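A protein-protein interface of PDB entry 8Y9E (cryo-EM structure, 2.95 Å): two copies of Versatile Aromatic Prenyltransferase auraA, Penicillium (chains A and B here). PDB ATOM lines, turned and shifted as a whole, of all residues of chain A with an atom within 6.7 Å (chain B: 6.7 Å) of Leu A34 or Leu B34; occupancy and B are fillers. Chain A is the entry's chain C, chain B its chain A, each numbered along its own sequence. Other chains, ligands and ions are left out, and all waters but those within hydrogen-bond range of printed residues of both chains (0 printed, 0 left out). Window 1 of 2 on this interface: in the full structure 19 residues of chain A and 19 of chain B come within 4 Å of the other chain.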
ATOM      1  N   PHE A  29       3.502 -21.267 -12.960  1.00  0.00           N
ATOM      2  CA  PHE A  29       2.901 -21.803 -14.172  1.00  0.00           C
ATOM      3  C   PHE A  29       3.773 -21.534 -15.389  1.00  0.00           C
ATOM      4  O   PHE A  29       3.927 -22.397 -16.262  1.00  0.00           O
ATOM      5  CB  PHE A  29       1.506 -21.207 -14.348  1.00  0.00           C
ATOM      6  CG  PHE A  29       0.804 -21.667 -15.572  1.00  0.00           C
ATOM      7  CD1 PHE A  29       0.318 -22.948 -15.662  1.00  0.00           C
ATOM      8  CD2 PHE A  29       0.625 -20.817 -16.637  1.00  0.00           C
ATOM      9  CE1 PHE A  29      -0.323 -23.371 -16.784  1.00  0.00           C
ATOM     10  CE2 PHE A  29      -0.017 -21.240 -17.760  1.00  0.00           C
ATOM     11  CZ  PHE A  29      -0.492 -22.521 -17.832  1.00  0.00           C
ATOM     12  N   LEU A  30       4.376 -20.350 -15.455  1.00  0.00           N
ATOM     13  CA  LEU A  30       5.193 -20.004 -16.607  1.00  0.00           C
ATOM     14  C   LEU A  30       6.488 -20.793 -16.618  1.00  0.00           C
ATOM     15  O   LEU A  30       6.950 -21.218 -17.679  1.00  0.00           O
ATOM     16  CB  LEU A  30       5.480 -18.511 -16.610  1.00  0.00           C
ATOM     17  CG  LEU A  30       4.356 -17.596 -17.058  1.00  0.00           C
ATOM     18  CD1 LEU A  30       4.706 -16.203 -16.738  1.00  0.00           C
ATOM     19  CD2 LEU A  30       4.135 -17.717 -18.512  1.00  0.00           C
ATOM     20  N   GLY A  31       7.098 -20.998 -15.454  1.00  0.00           N
ATOM     21  CA  GLY A  31       8.268 -21.849 -15.398  1.00  0.00           C
ATOM     22  C   GLY A  31       7.945 -23.278 -15.754  1.00  0.00           C
ATOM     23  O   GLY A  31       8.822 -24.032 -16.184  1.00  0.00           O
ATOM     24  N   ARG A  32       6.685 -23.669 -15.583  1.00  0.00           N
ATOM     25  CA  ARG A  32       6.284 -25.020 -15.943  1.00  0.00           C
ATOM     26  C   ARG A  32       6.082 -25.163 -17.445  1.00  0.00           C
ATOM     27  O   ARG A  32       6.531 -26.150 -18.039  1.00  0.00           O
ATOM     28  CB  ARG A  32       5.009 -25.398 -15.196  1.00  0.00           C
ATOM     29  CG  ARG A  32       5.200 -25.565 -13.709  1.00  0.00           C
ATOM     30  CD  ARG A  32       4.336 -26.651 -13.149  1.00  0.00           C
ATOM     31  NE  ARG A  32       2.961 -26.210 -12.969  1.00  0.00           N
ATOM     32  CZ  ARG A  32       2.461 -25.759 -11.826  1.00  0.00           C
ATOM     33  NH1 ARG A  32       3.216 -25.675 -10.745  1.00  0.00           N
ATOM     34  NH2 ARG A  32       1.195 -25.384 -11.770  1.00  0.00           N
ATOM     35  N   VAL A  33       5.426 -24.194 -18.077  1.00  0.00           N
ATOM     36  CA  VAL A  33       5.086 -24.331 -19.487  1.00  0.00           C
ATOM     37  C   VAL A  33       6.145 -23.751 -20.420  1.00  0.00           C
ATOM     38  O   VAL A  33       6.283 -24.216 -21.554  1.00  0.00           O
ATOM     39  CB  VAL A  33       3.722 -23.688 -19.765  1.00  0.00           C
ATOM     40  CG1 VAL A  33       2.709 -24.154 -18.774  1.00  0.00           C
ATOM     41  CG2 VAL A  33       3.831 -22.224 -19.717  1.00  0.00           C
ATOM     42  N   LEU A  34       6.895 -22.750 -19.983  1.00  0.00           N
ATOM     43  CA  LEU A  34       7.741 -22.008 -20.903  1.00  0.00           C
ATOM     44  C   LEU A  34       8.959 -22.819 -21.307  1.00  0.00           C
ATOM     45  O   LEU A  34       9.525 -23.567 -20.507  1.00  0.00           O
ATOM     46  CB  LEU A  34       8.194 -20.692 -20.286  1.00  0.00           C
ATOM     47  CG  LEU A  34       7.194 -19.553 -20.178  1.00  0.00           C
ATOM     48  CD1 LEU A  34       7.876 -18.384 -19.579  1.00  0.00           C
ATOM     49  CD2 LEU A  34       6.639 -19.186 -21.511  1.00  0.00           C
ATOM     50  N   GLN A  35       9.359 -22.660 -22.562  1.00  0.00           N
ATOM     51  CA  GLN A  35      10.572 -23.261 -23.079  1.00  0.00           C
ATOM     52  C   GLN A  35      11.656 -22.199 -23.121  1.00  0.00           C
ATOM     53  O   GLN A  35      11.445 -21.111 -23.663  1.00  0.00           O
ATOM     54  CB  GLN A  35      10.340 -23.846 -24.472  1.00  0.00           C
ATOM     55  CG  GLN A  35      10.011 -25.326 -24.498  1.00  0.00           C
ATOM     56  CD  GLN A  35       8.544 -25.598 -24.249  1.00  0.00           C
ATOM     57  OE1 GLN A  35       7.675 -24.974 -24.853  1.00  0.00           O
ATOM     58  NE2 GLN A  35       8.261 -26.520 -23.342  1.00  0.00           N
ATOM     59  N   PHE A  36      12.803 -22.511 -22.535  1.00  0.00           N
ATOM     60  CA  PHE A  36      13.900 -21.572 -22.406  1.00  0.00           C
ATOM     61  C   PHE A  36      15.016 -21.926 -23.375  1.00  0.00           C
ATOM     62  O   PHE A  36      15.409 -23.089 -23.486  1.00  0.00           O
ATOM     63  CB  PHE A  36      14.433 -21.572 -20.981  1.00  0.00           C
ATOM     64  CG  PHE A  36      13.465 -21.051 -19.969  1.00  0.00           C
ATOM     65  CD1 PHE A  36      13.365 -19.706 -19.709  1.00  0.00           C
ATOM     66  CD2 PHE A  36      12.667 -21.909 -19.262  1.00  0.00           C
ATOM     67  CE1 PHE A  36      12.489 -19.243 -18.781  1.00  0.00           C
ATOM     68  CE2 PHE A  36      11.787 -21.437 -18.334  1.00  0.00           C
ATOM     69  CZ  PHE A  36      11.702 -20.109 -18.097  1.00  0.00           C
ATOM     70  N   LYS A  42      16.751 -20.300 -17.480  1.00  0.00           N
ATOM     71  CA  LYS A  42      15.889 -21.024 -16.556  1.00  0.00           C
ATOM     72  C   LYS A  42      16.267 -20.729 -15.113  1.00  0.00           C
ATOM     73  O   LYS A  42      15.392 -20.543 -14.259  1.00  0.00           O
ATOM     74  CB  LYS A  42      15.977 -22.520 -16.844  1.00  0.00           C
ATOM     75  CG  LYS A  42      15.230 -23.396 -15.883  1.00  0.00           C
ATOM     76  CD  LYS A  42      13.790 -22.985 -15.746  1.00  0.00           C
ATOM     77  CE  LYS A  42      13.057 -23.882 -14.795  1.00  0.00           C
ATOM     78  NZ  LYS A  42      11.634 -23.523 -14.708  1.00  0.00           N
ATOM     79  N   TRP A  45      15.341 -17.278 -14.170  1.00  0.00           N
ATOM     80  CA  TRP A  45      13.905 -17.254 -13.945  1.00  0.00           C
ATOM     81  C   TRP A  45      13.582 -17.745 -12.548  1.00  0.00           C
ATOM     82  O   TRP A  45      12.949 -17.036 -11.760  1.00  0.00           O
ATOM     83  CB  TRP A  45      13.194 -18.107 -14.992  1.00  0.00           C
ATOM     84  CG  TRP A  45      11.727 -18.150 -14.792  1.00  0.00           C
ATOM     85  CD1 TRP A  45      11.038 -19.010 -14.004  1.00  0.00           C
ATOM     86  CD2 TRP A  45      10.758 -17.282 -15.378  1.00  0.00           C
ATOM     87  NE1 TRP A  45       9.703 -18.737 -14.059  1.00  0.00           N
ATOM     88  CE2 TRP A  45       9.506 -17.676 -14.898  1.00  0.00           C
ATOM     89  CE3 TRP A  45      10.830 -16.209 -16.262  1.00  0.00           C
ATOM     90  CZ2 TRP A  45       8.342 -17.041 -15.271  1.00  0.00           C
ATOM     91  CZ3 TRP A  45       9.674 -15.587 -16.627  1.00  0.00           C
ATOM     92  CH2 TRP A  45       8.448 -16.001 -16.136  1.00  0.00           C
ATOM     93  N   LEU A  70       6.322 -10.764 -16.898  1.00  0.00           N
ATOM     94  CA  LEU A  70       7.172 -11.928 -16.725  1.00  0.00           C
ATOM     95  C   LEU A  70       7.589 -12.504 -18.066  1.00  0.00           C
ATOM     96  O   LEU A  70       8.710 -12.993 -18.206  1.00  0.00           O
ATOM     97  CB  LEU A  70       6.447 -12.964 -15.881  1.00  0.00           C
ATOM     98  CG  LEU A  70       6.222 -12.534 -14.438  1.00  0.00           C
ATOM     99  CD1 LEU A  70       5.256 -13.426 -13.755  1.00  0.00           C
ATOM    100  CD2 LEU A  70       7.508 -12.543 -13.704  1.00  0.00           C
ATOM    101  N   LEU A  71       6.732 -12.407 -19.075  1.00  0.00           N
ATOM    102  CA  LEU A  71       7.114 -12.853 -20.405  1.00  0.00           C
ATOM    103  C   LEU A  71       8.097 -11.896 -21.061  1.00  0.00           C
ATOM    104  O   LEU A  71       8.989 -12.333 -21.793  1.00  0.00           O
ATOM    105  CB  LEU A  71       5.868 -13.010 -21.262  1.00  0.00           C
ATOM    106  CG  LEU A  71       5.040 -14.247 -20.963  1.00  0.00           C
ATOM    107  CD1 LEU A  71       3.631 -14.021 -21.383  1.00  0.00           C
ATOM    108  CD2 LEU A  71       5.623 -15.427 -21.668  1.00  0.00           C
ATOM    109  N   TYR A  74      11.214 -12.806 -19.631  1.00  0.00           N
ATOM    110  CA  TYR A  74      11.662 -14.092 -20.149  1.00  0.00           C
ATOM    111  C   TYR A  74      12.273 -13.958 -21.535  1.00  0.00           C
ATOM    112  O   TYR A  74      13.223 -14.672 -21.870  1.00  0.00           O
ATOM    113  CB  TYR A  74      10.484 -15.061 -20.155  1.00  0.00           C
ATOM    114  CG  TYR A  74      10.489 -16.106 -21.237  1.00  0.00           C
ATOM    115  CD1 TYR A  74      11.346 -17.185 -21.187  1.00  0.00           C
ATOM    116  CD2 TYR A  74       9.611 -16.030 -22.295  1.00  0.00           C
ATOM    117  CE1 TYR A  74      11.334 -18.137 -22.171  1.00  0.00           C
ATOM    118  CE2 TYR A  74       9.599 -16.974 -23.272  1.00  0.00           C
ATOM    119  CZ  TYR A  74      10.460 -18.025 -23.208  1.00  0.00           C
ATOM    120  OH  TYR A  74      10.449 -18.979 -24.186  1.00  0.00           O
ATOM    121  N   ASP A  75      11.754 -13.045 -22.351  1.00  0.00           N
ATOM    122  CA  ASP A  75      12.206 -12.884 -23.726  1.00  0.00           C
ATOM    123  C   ASP A  75      13.262 -11.801 -23.878  1.00  0.00           C
ATOM    124  O   ASP A  75      14.327 -12.043 -24.447  1.00  0.00           O
ATOM    125  CB  ASP A  75      11.020 -12.557 -24.630  1.00  0.00           C
ATOM    126  CG  ASP A  75      11.269 -12.935 -26.070  1.00  0.00           C
ATOM    127  OD1 ASP A  75      11.455 -14.138 -26.350  1.00  0.00           O
ATOM    128  OD2 ASP A  75      11.280 -12.029 -26.928  1.00  0.00           O
ATOM    129  N   ARG A 146      14.420  -6.042 -28.707  1.00  0.00           N
ATOM    130  CA  ARG A 146      13.324  -6.867 -28.218  1.00  0.00           C
ATOM    131  C   ARG A 146      12.218  -6.013 -27.620  1.00  0.00           C
ATOM    132  O   ARG A 146      11.037  -6.249 -27.888  1.00  0.00           O
ATOM    133  CB  ARG A 146      13.829  -7.870 -27.188  1.00  0.00           C
ATOM    134  CG  ARG A 146      14.775  -8.936 -27.706  1.00  0.00           C
ATOM    135  CD  ARG A 146      14.194  -9.720 -28.849  1.00  0.00           C
ATOM    136  NE  ARG A 146      12.902 -10.301 -28.511  1.00  0.00           N
ATOM    137  CZ  ARG A 146      11.905 -10.457 -29.372  1.00  0.00           C
ATOM    138  NH1 ARG A 146      12.034 -10.084 -30.633  1.00  0.00           N
ATOM    139  NH2 ARG A 146      10.769 -10.990 -28.970  1.00  0.00           N
ATOM    140  N   PHE B  29       0.747 -11.237 -28.514  1.00  0.00           N
ATOM    141  CA  PHE B  29       1.875 -11.040 -27.614  1.00  0.00           C
ATOM    142  C   PHE B  29       2.608 -12.347 -27.350  1.00  0.00           C
ATOM    143  O   PHE B  29       3.844 -12.380 -27.303  1.00  0.00           O
ATOM    144  CB  PHE B  29       1.375 -10.413 -26.314  1.00  0.00           C
ATOM    145  CG  PHE B  29       2.442 -10.188 -25.305  1.00  0.00           C
ATOM    146  CD1 PHE B  29       3.375  -9.195 -25.482  1.00  0.00           C
ATOM    147  CD2 PHE B  29       2.514 -10.967 -24.177  1.00  0.00           C
ATOM    148  CE1 PHE B  29       4.353  -8.990 -24.561  1.00  0.00           C
ATOM    149  CE2 PHE B  29       3.494 -10.761 -23.255  1.00  0.00           C
ATOM    150  CZ  PHE B  29       4.414  -9.769 -23.449  1.00  0.00           C
ATOM    151  N   LEU B  30       1.865 -13.441 -27.201  1.00  0.00           N
ATOM    152  CA  LEU B  30       2.491 -14.720 -26.906  1.00  0.00           C
ATOM    153  C   LEU B  30       3.243 -15.253 -28.112  1.00  0.00           C
ATOM    154  O   LEU B  30       4.325 -15.826 -27.967  1.00  0.00           O
ATOM    155  CB  LEU B  30       1.442 -15.719 -26.450  1.00  0.00           C
ATOM    156  CG  LEU B  30       0.928 -15.576 -25.030  1.00  0.00           C
ATOM    157  CD1 LEU B  30      -0.258 -16.427 -24.851  1.00  0.00           C
ATOM    158  CD2 LEU B  30       1.963 -15.980 -24.058  1.00  0.00           C
ATOM    159  N   GLY B  31       2.690 -15.086 -29.309  1.00  0.00           N
ATOM    160  CA  GLY B  31       3.426 -15.466 -30.496  1.00  0.00           C
ATOM    161  C   GLY B  31       4.665 -14.630 -30.685  1.00  0.00           C
ATOM    162  O   GLY B  31       5.618 -15.059 -31.342  1.00  0.00           O
ATOM    163  N   ARG B  32       4.674 -13.429 -30.113  1.00  0.00           N
ATOM    164  CA  ARG B  32       5.850 -12.579 -30.214  1.00  0.00           C
ATOM    165  C   ARG B  32       6.936 -13.007 -29.238  1.00  0.00           C
ATOM    166  O   ARG B  32       8.113 -13.071 -29.609  1.00  0.00           O
ATOM    167  CB  ARG B  32       5.459 -11.125 -29.972  1.00  0.00           C
ATOM    168  CG  ARG B  32       4.607 -10.532 -31.066  1.00  0.00           C
ATOM    169  CD  ARG B  32       4.912  -9.085 -31.296  1.00  0.00           C
ATOM    170  NE  ARG B  32       4.291  -8.236 -30.289  1.00  0.00           N
ATOM    171  CZ  ARG B  32       3.130  -7.613 -30.446  1.00  0.00           C
ATOM    172  NH1 ARG B  32       2.440  -7.741 -31.567  1.00  0.00           N
ATOM    173  NH2 ARG B  32       2.654  -6.862 -29.468  1.00  0.00           N
ATOM    174  N   VAL B  33       6.567 -13.314 -27.997  1.00  0.00           N
ATOM    175  CA  VAL B  33       7.569 -13.604 -26.979  1.00  0.00           C
ATOM    176  C   VAL B  33       7.910 -15.088 -26.877  1.00  0.00           C
ATOM    177  O   VAL B  33       9.028 -15.435 -26.489  1.00  0.00           O
ATOM    178  CB  VAL B  33       7.110 -13.068 -25.619  1.00  0.00           C
ATOM    179  CG1 VAL B  33       6.654 -11.653 -25.737  1.00  0.00           C
ATOM    180  CG2 VAL B  33       6.023 -13.900 -25.086  1.00  0.00           C
ATOM    181  N   LEU B  34       6.982 -15.975 -27.209  1.00  0.00           N
ATOM    182  CA  LEU B  34       7.169 -17.384 -26.900  1.00  0.00           C
ATOM    183  C   LEU B  34       8.190 -18.019 -27.827  1.00  0.00           C
ATOM    184  O   LEU B  34       8.272 -17.692 -29.012  1.00  0.00           O
ATOM    185  CB  LEU B  34       5.853 -18.142 -27.005  1.00  0.00           C
ATOM    186  CG  LEU B  34       4.819 -17.967 -25.905  1.00  0.00           C
ATOM    187  CD1 LEU B  34       3.652 -18.822 -26.215  1.00  0.00           C
ATOM    188  CD2 LEU B  34       5.374 -18.332 -24.571  1.00  0.00           C
ATOM    189  N   GLN B  35       8.967 -18.939 -27.271  1.00  0.00           N
ATOM    190  CA  GLN B  35       9.911 -19.732 -28.034  1.00  0.00           C
ATOM    191  C   GLN B  35       9.304 -21.102 -28.276  1.00  0.00           C
ATOM    192  O   GLN B  35       8.846 -21.758 -27.336  1.00  0.00           O
ATOM    193  CB  GLN B  35      11.242 -19.858 -27.295  1.00  0.00           C
ATOM    194  CG  GLN B  35      12.298 -18.847 -27.702  1.00  0.00           C
ATOM    195  CD  GLN B  35      12.137 -17.524 -26.985  1.00  0.00           C
ATOM    196  OE1 GLN B  35      11.976 -17.481 -25.768  1.00  0.00           O
ATOM    197  NE2 GLN B  35      12.166 -16.437 -27.740  1.00  0.00           N
ATOM    198  N   PHE B  36       9.288 -21.521 -29.533  1.00  0.00           N
ATOM    199  CA  PHE B  36       8.657 -22.763 -29.938  1.00  0.00           C
ATOM    200  C   PHE B  36       9.710 -23.810 -30.258  1.00  0.00           C
ATOM    201  O   PHE B  36      10.685 -23.531 -30.959  1.00  0.00           O
ATOM    202  CB  PHE B  36       7.770 -22.534 -31.153  1.00  0.00           C
ATOM    203  CG  PHE B  36       6.584 -21.663 -30.887  1.00  0.00           C
ATOM    204  CD1 PHE B  36       5.416 -22.189 -30.393  1.00  0.00           C
ATOM    205  CD2 PHE B  36       6.634 -20.322 -31.148  1.00  0.00           C
ATOM    206  CE1 PHE B  36       4.342 -21.391 -30.161  1.00  0.00           C
ATOM    207  CE2 PHE B  36       5.552 -19.527 -30.912  1.00  0.00           C
ATOM    208  CZ  PHE B  36       4.412 -20.063 -30.421  1.00  0.00           C
ATOM    209  N   LYS B  42       4.792 -23.381 -34.262  1.00  0.00           N
ATOM    210  CA  LYS B  42       4.589 -21.969 -34.554  1.00  0.00           C
ATOM    211  C   LYS B  42       3.453 -21.775 -35.547  1.00  0.00           C
ATOM    212  O   LYS B  42       2.631 -20.865 -35.394  1.00  0.00           O
ATOM    213  CB  LYS B  42       5.885 -21.368 -35.088  1.00  0.00           C
ATOM    214  CG  LYS B  42       5.784 -19.943 -35.546  1.00  0.00           C
ATOM    215  CD  LYS B  42       5.205 -19.050 -34.484  1.00  0.00           C
ATOM    216  CE  LYS B  42       5.126 -17.628 -34.954  1.00  0.00           C
ATOM    217  NZ  LYS B  42       4.621 -16.742 -33.895  1.00  0.00           N
ATOM    218  N   TRP B  45       0.181 -22.513 -33.996  1.00  0.00           N
ATOM    219  CA  TRP B  45      -0.172 -21.381 -33.157  1.00  0.00           C
ATOM    220  C   TRP B  45      -0.795 -20.280 -33.994  1.00  0.00           C
ATOM    221  O   TRP B  45      -1.922 -19.851 -33.736  1.00  0.00           O
ATOM    222  CB  TRP B  45       1.061 -20.864 -32.421  1.00  0.00           C
ATOM    223  CG  TRP B  45       0.768 -19.683 -31.575  1.00  0.00           C
ATOM    224  CD1 TRP B  45       0.779 -18.384 -31.960  1.00  0.00           C
ATOM    225  CD2 TRP B  45       0.401 -19.689 -30.198  1.00  0.00           C
ATOM    226  NE1 TRP B  45       0.441 -17.577 -30.914  1.00  0.00           N
ATOM    227  CE2 TRP B  45       0.205 -18.358 -29.816  1.00  0.00           C
ATOM    228  CE3 TRP B  45       0.221 -20.690 -29.248  1.00  0.00           C
ATOM    229  CZ2 TRP B  45      -0.159 -18.004 -28.535  1.00  0.00           C
ATOM    230  CZ3 TRP B  45      -0.138 -20.333 -27.982  1.00  0.00           C
ATOM    231  CH2 TRP B  45      -0.323 -19.006 -27.635  1.00  0.00           C
ATOM    232  N   LEU B  70      -3.911 -20.550 -23.479  1.00  0.00           N
ATOM    233  CA  LEU B  70      -3.066 -20.481 -24.657  1.00  0.00           C
ATOM    234  C   LEU B  70      -1.693 -21.062 -24.380  1.00  0.00           C
ATOM    235  O   LEU B  70      -1.095 -21.683 -25.260  1.00  0.00           O
ATOM    236  CB  LEU B  70      -2.972 -19.039 -25.129  1.00  0.00           C
ATOM    237  CG  LEU B  70      -4.282 -18.477 -25.659  1.00  0.00           C
ATOM    238  CD1 LEU B  70      -4.216 -17.004 -25.810  1.00  0.00           C
ATOM    239  CD2 LEU B  70      -4.602 -19.092 -26.967  1.00  0.00           C
ATOM    240  N   LEU B  71      -1.198 -20.925 -23.157  1.00  0.00           N
ATOM    241  CA  LEU B  71       0.070 -21.545 -22.807  1.00  0.00           C
ATOM    242  C   LEU B  71      -0.060 -23.052 -22.656  1.00  0.00           C
ATOM    243  O   LEU B  71       0.866 -23.790 -23.004  1.00  0.00           O
ATOM    244  CB  LEU B  71       0.599 -20.923 -21.524  1.00  0.00           C
ATOM    245  CG  LEU B  71       1.194 -19.536 -21.685  1.00  0.00           C
ATOM    246  CD1 LEU B  71       1.128 -18.808 -20.390  1.00  0.00           C
ATOM    247  CD2 LEU B  71       2.604 -19.643 -22.165  1.00  0.00           C
ATOM    248  N   TYR B  74       0.049 -24.228 -26.002  1.00  0.00           N
ATOM    249  CA  TYR B  74       1.393 -24.100 -26.550  1.00  0.00           C
ATOM    250  C   TYR B  74       2.304 -25.219 -26.067  1.00  0.00           C
ATOM    251  O   TYR B  74       3.174 -25.681 -26.813  1.00  0.00           O
ATOM    252  CB  TYR B  74       1.952 -22.732 -26.176  1.00  0.00           C
ATOM    253  CG  TYR B  74       3.441 -22.652 -25.983  1.00  0.00           C
ATOM    254  CD1 TYR B  74       4.306 -22.686 -27.055  1.00  0.00           C
ATOM    255  CD2 TYR B  74       3.981 -22.508 -24.724  1.00  0.00           C
ATOM    256  CE1 TYR B  74       5.660 -22.601 -26.869  1.00  0.00           C
ATOM    257  CE2 TYR B  74       5.324 -22.425 -24.538  1.00  0.00           C
ATOM    258  CZ  TYR B  74       6.160 -22.471 -25.610  1.00  0.00           C
ATOM    259  OH  TYR B  74       7.511 -22.383 -25.427  1.00  0.00           O
ATOM    260  N   ASP B  75       2.119 -25.675 -24.832  1.00  0.00           N
ATOM    261  CA  ASP B  75       2.982 -26.686 -24.239  1.00  0.00           C
ATOM    262  C   ASP B  75       2.430 -28.095 -24.385  1.00  0.00           C
ATOM    263  O   ASP B  75       3.127 -28.992 -24.863  1.00  0.00           O
ATOM    264  CB  ASP B  75       3.196 -26.384 -22.757  1.00  0.00           C
ATOM    265  CG  ASP B  75       4.472 -26.991 -22.223  1.00  0.00           C
ATOM    266  OD1 ASP B  75       5.561 -26.612 -22.701  1.00  0.00           O
ATOM    267  OD2 ASP B  75       4.387 -27.849 -21.321  1.00  0.00           O
ATOM    268  N   ARG B 146       1.618 -34.075 -19.758  1.00  0.00           N
ATOM    269  CA  ARG B 146       1.750 -32.626 -19.676  1.00  0.00           C
ATOM    270  C   ARG B 146       0.582 -32.010 -18.922  1.00  0.00           C
ATOM    271  O   ARG B 146       0.781 -31.140 -18.072  1.00  0.00           O
ATOM    272  CB  ARG B 146       1.855 -32.019 -21.069  1.00  0.00           C
ATOM    273  CG  ARG B 146       3.106 -32.371 -21.855  1.00  0.00           C
ATOM    274  CD  ARG B 146       4.368 -32.028 -21.118  1.00  0.00           C
ATOM    275  NE  ARG B 146       4.398 -30.633 -20.707  1.00  0.00           N
ATOM    276  CZ  ARG B 146       4.960 -30.195 -19.587  1.00  0.00           C
ATOM    277  NH1 ARG B 146       5.552 -31.032 -18.754  1.00  0.00           N
ATOM    278  NH2 ARG B 146       4.932 -28.909 -19.298  1.00  0.00           N
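Phe A29 touches Leu B71 (CE2 to CD1, 3.8 Å).
Leu B71 touches Leu A30 (CD1 to CD2, 3.7 Å).
Leu B71 touches Val A33.
Val A33 touches Tyr B74 (O to CE2, 3.6 Å).
Leu A34 touches Leu B34.
Gln B35 touches Gln A35 (O to CB, 3.8 Å).
CD1 of Leu A71 touches CE2 of Phe B29, at 3.8 Å.
Leu A71 touches Leu B30 (CD1 to CD2, 3.7 Å).
CG2 of Val B33 touches CD2 of Leu A71, at 3.8 Å.
O of Val B33 touches CE2 of Tyr A74 (3.6 Å).
Leu B34 touches just one residue of chain A: Leu A34.
Of the printed residues of chain A, Val B33 touches Leu A71, Tyr A74 and Asp A75.
Of the printed residues of chain B, Arg A146 touches Arg B32 (3.4 Å).
Of the printed residues of chain A, Leu B71 touches Phe A29, Leu A30 and Val A33.
Of the printed residues of chain A, Phe B29 touches Leu A71.
Of the printed residues of chain A, Arg B32 touches Arg A146.
Lys A42 touches none of the printed residues of chain B.
Lys B42 touches none of the printed residues of chain A.
The nearest residue of chain B that does not touch Leu A34 is Leu B71 (4.1 Å).
The nearest residue of chain A that does not touch Leu B34 is Leu A71 (4.1 Å).
O of Gln B35 sits at hydrogen-bond distance from OH of Tyr B74.
OD2 of Asp B75 is in salt-bridge range of NE of Arg B146.
The backbone carbonyl oxygen of Gln A35 sits at hydrogen-bond distance from the side-chain hydroxyl of Tyr A74 (2.4 Å).
The guanidinium group (NE) of Arg A146 lies within salt-bridge range of the side-chain carboxylate (OD2) of Asp A75 (2.9 Å).
O of Arg B32 sits at hydrogen-bond distance from NH2 of Arg A146.
The side-chain amide oxygen of Gln B35 sits at hydrogen-bond distance from the side-chain hydroxyl of Tyr A74.
NE2 of Gln B35 lies within hydrogen-bond range of OD1 of Asp A75 (2.8 Å).
The side-chain hydroxyl (OH) of Tyr B74 lies within hydrogen-bond range of the side-chain amide oxygen (OE1) of Gln A35.
The side-chain amide nitrogen of Gln A35 is in hydrogen-bond range of the side-chain carboxylate of Asp B75 (2.8 Å).
NH2 of Arg B146 lies within hydrogen-bond range of O of Arg A32, 3.4 Å away.
The side-chain carboxylate (OD1) of Asp B75 sits close to the backbone carbonyl oxygen (O) of Val A33.
The side-chain carboxylate (OD1) of Asp A75 sits close to the backbone carbonyl oxygen (O) of Val B33 (2.8 Å).
Phe A29 touches Leu B71, and with the chains exchanged Leu A71 touches Phe B29.
Leu A30 touches Leu B71, and with the chains exchanged Leu A71 touches Leu B30.
Gln B35 touches its own counterpart, Gln A35.
Gln A35 touches Asp B75, and with the chains exchanged Asp A75 touches Gln B35.
Positions printed for both chains: 29, 30, 31, 32, 33, 34, 35, 36, 42, 45, 70, 71, 74, 75 and 146.
Of the 18 pairs that touch across the chains among the printed residues, 18 have their exchanged pair printed and touching as well.
Printed residues of chain A that touch a printed residue of chain B: Phe A29, Leu A30, Arg A32, Val A33, Leu A34, Gln A35, Leu A71, Tyr A74, Asp A75 and Arg A146.
Hydrophobic or aromatic side chains of chain A that line the printed part of chain B: Phe A29, Leu A30, Val A33, Leu A34, Leu A71 and Tyr A74.
Printed residues of chain B that touch a printed residue of chain A: Phe B29, Leu B30, Arg B32, Val B33, Leu B34, Gln B35, Leu B71, Tyr B74, Asp B75 and Arg B146.
Among the printed residues, 18 pairs touch across the chains.
Among the printed residues, no Asp or Glu carboxylate lies within 4 Å of a Lys or Arg side-chain nitrogen of the other chain.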
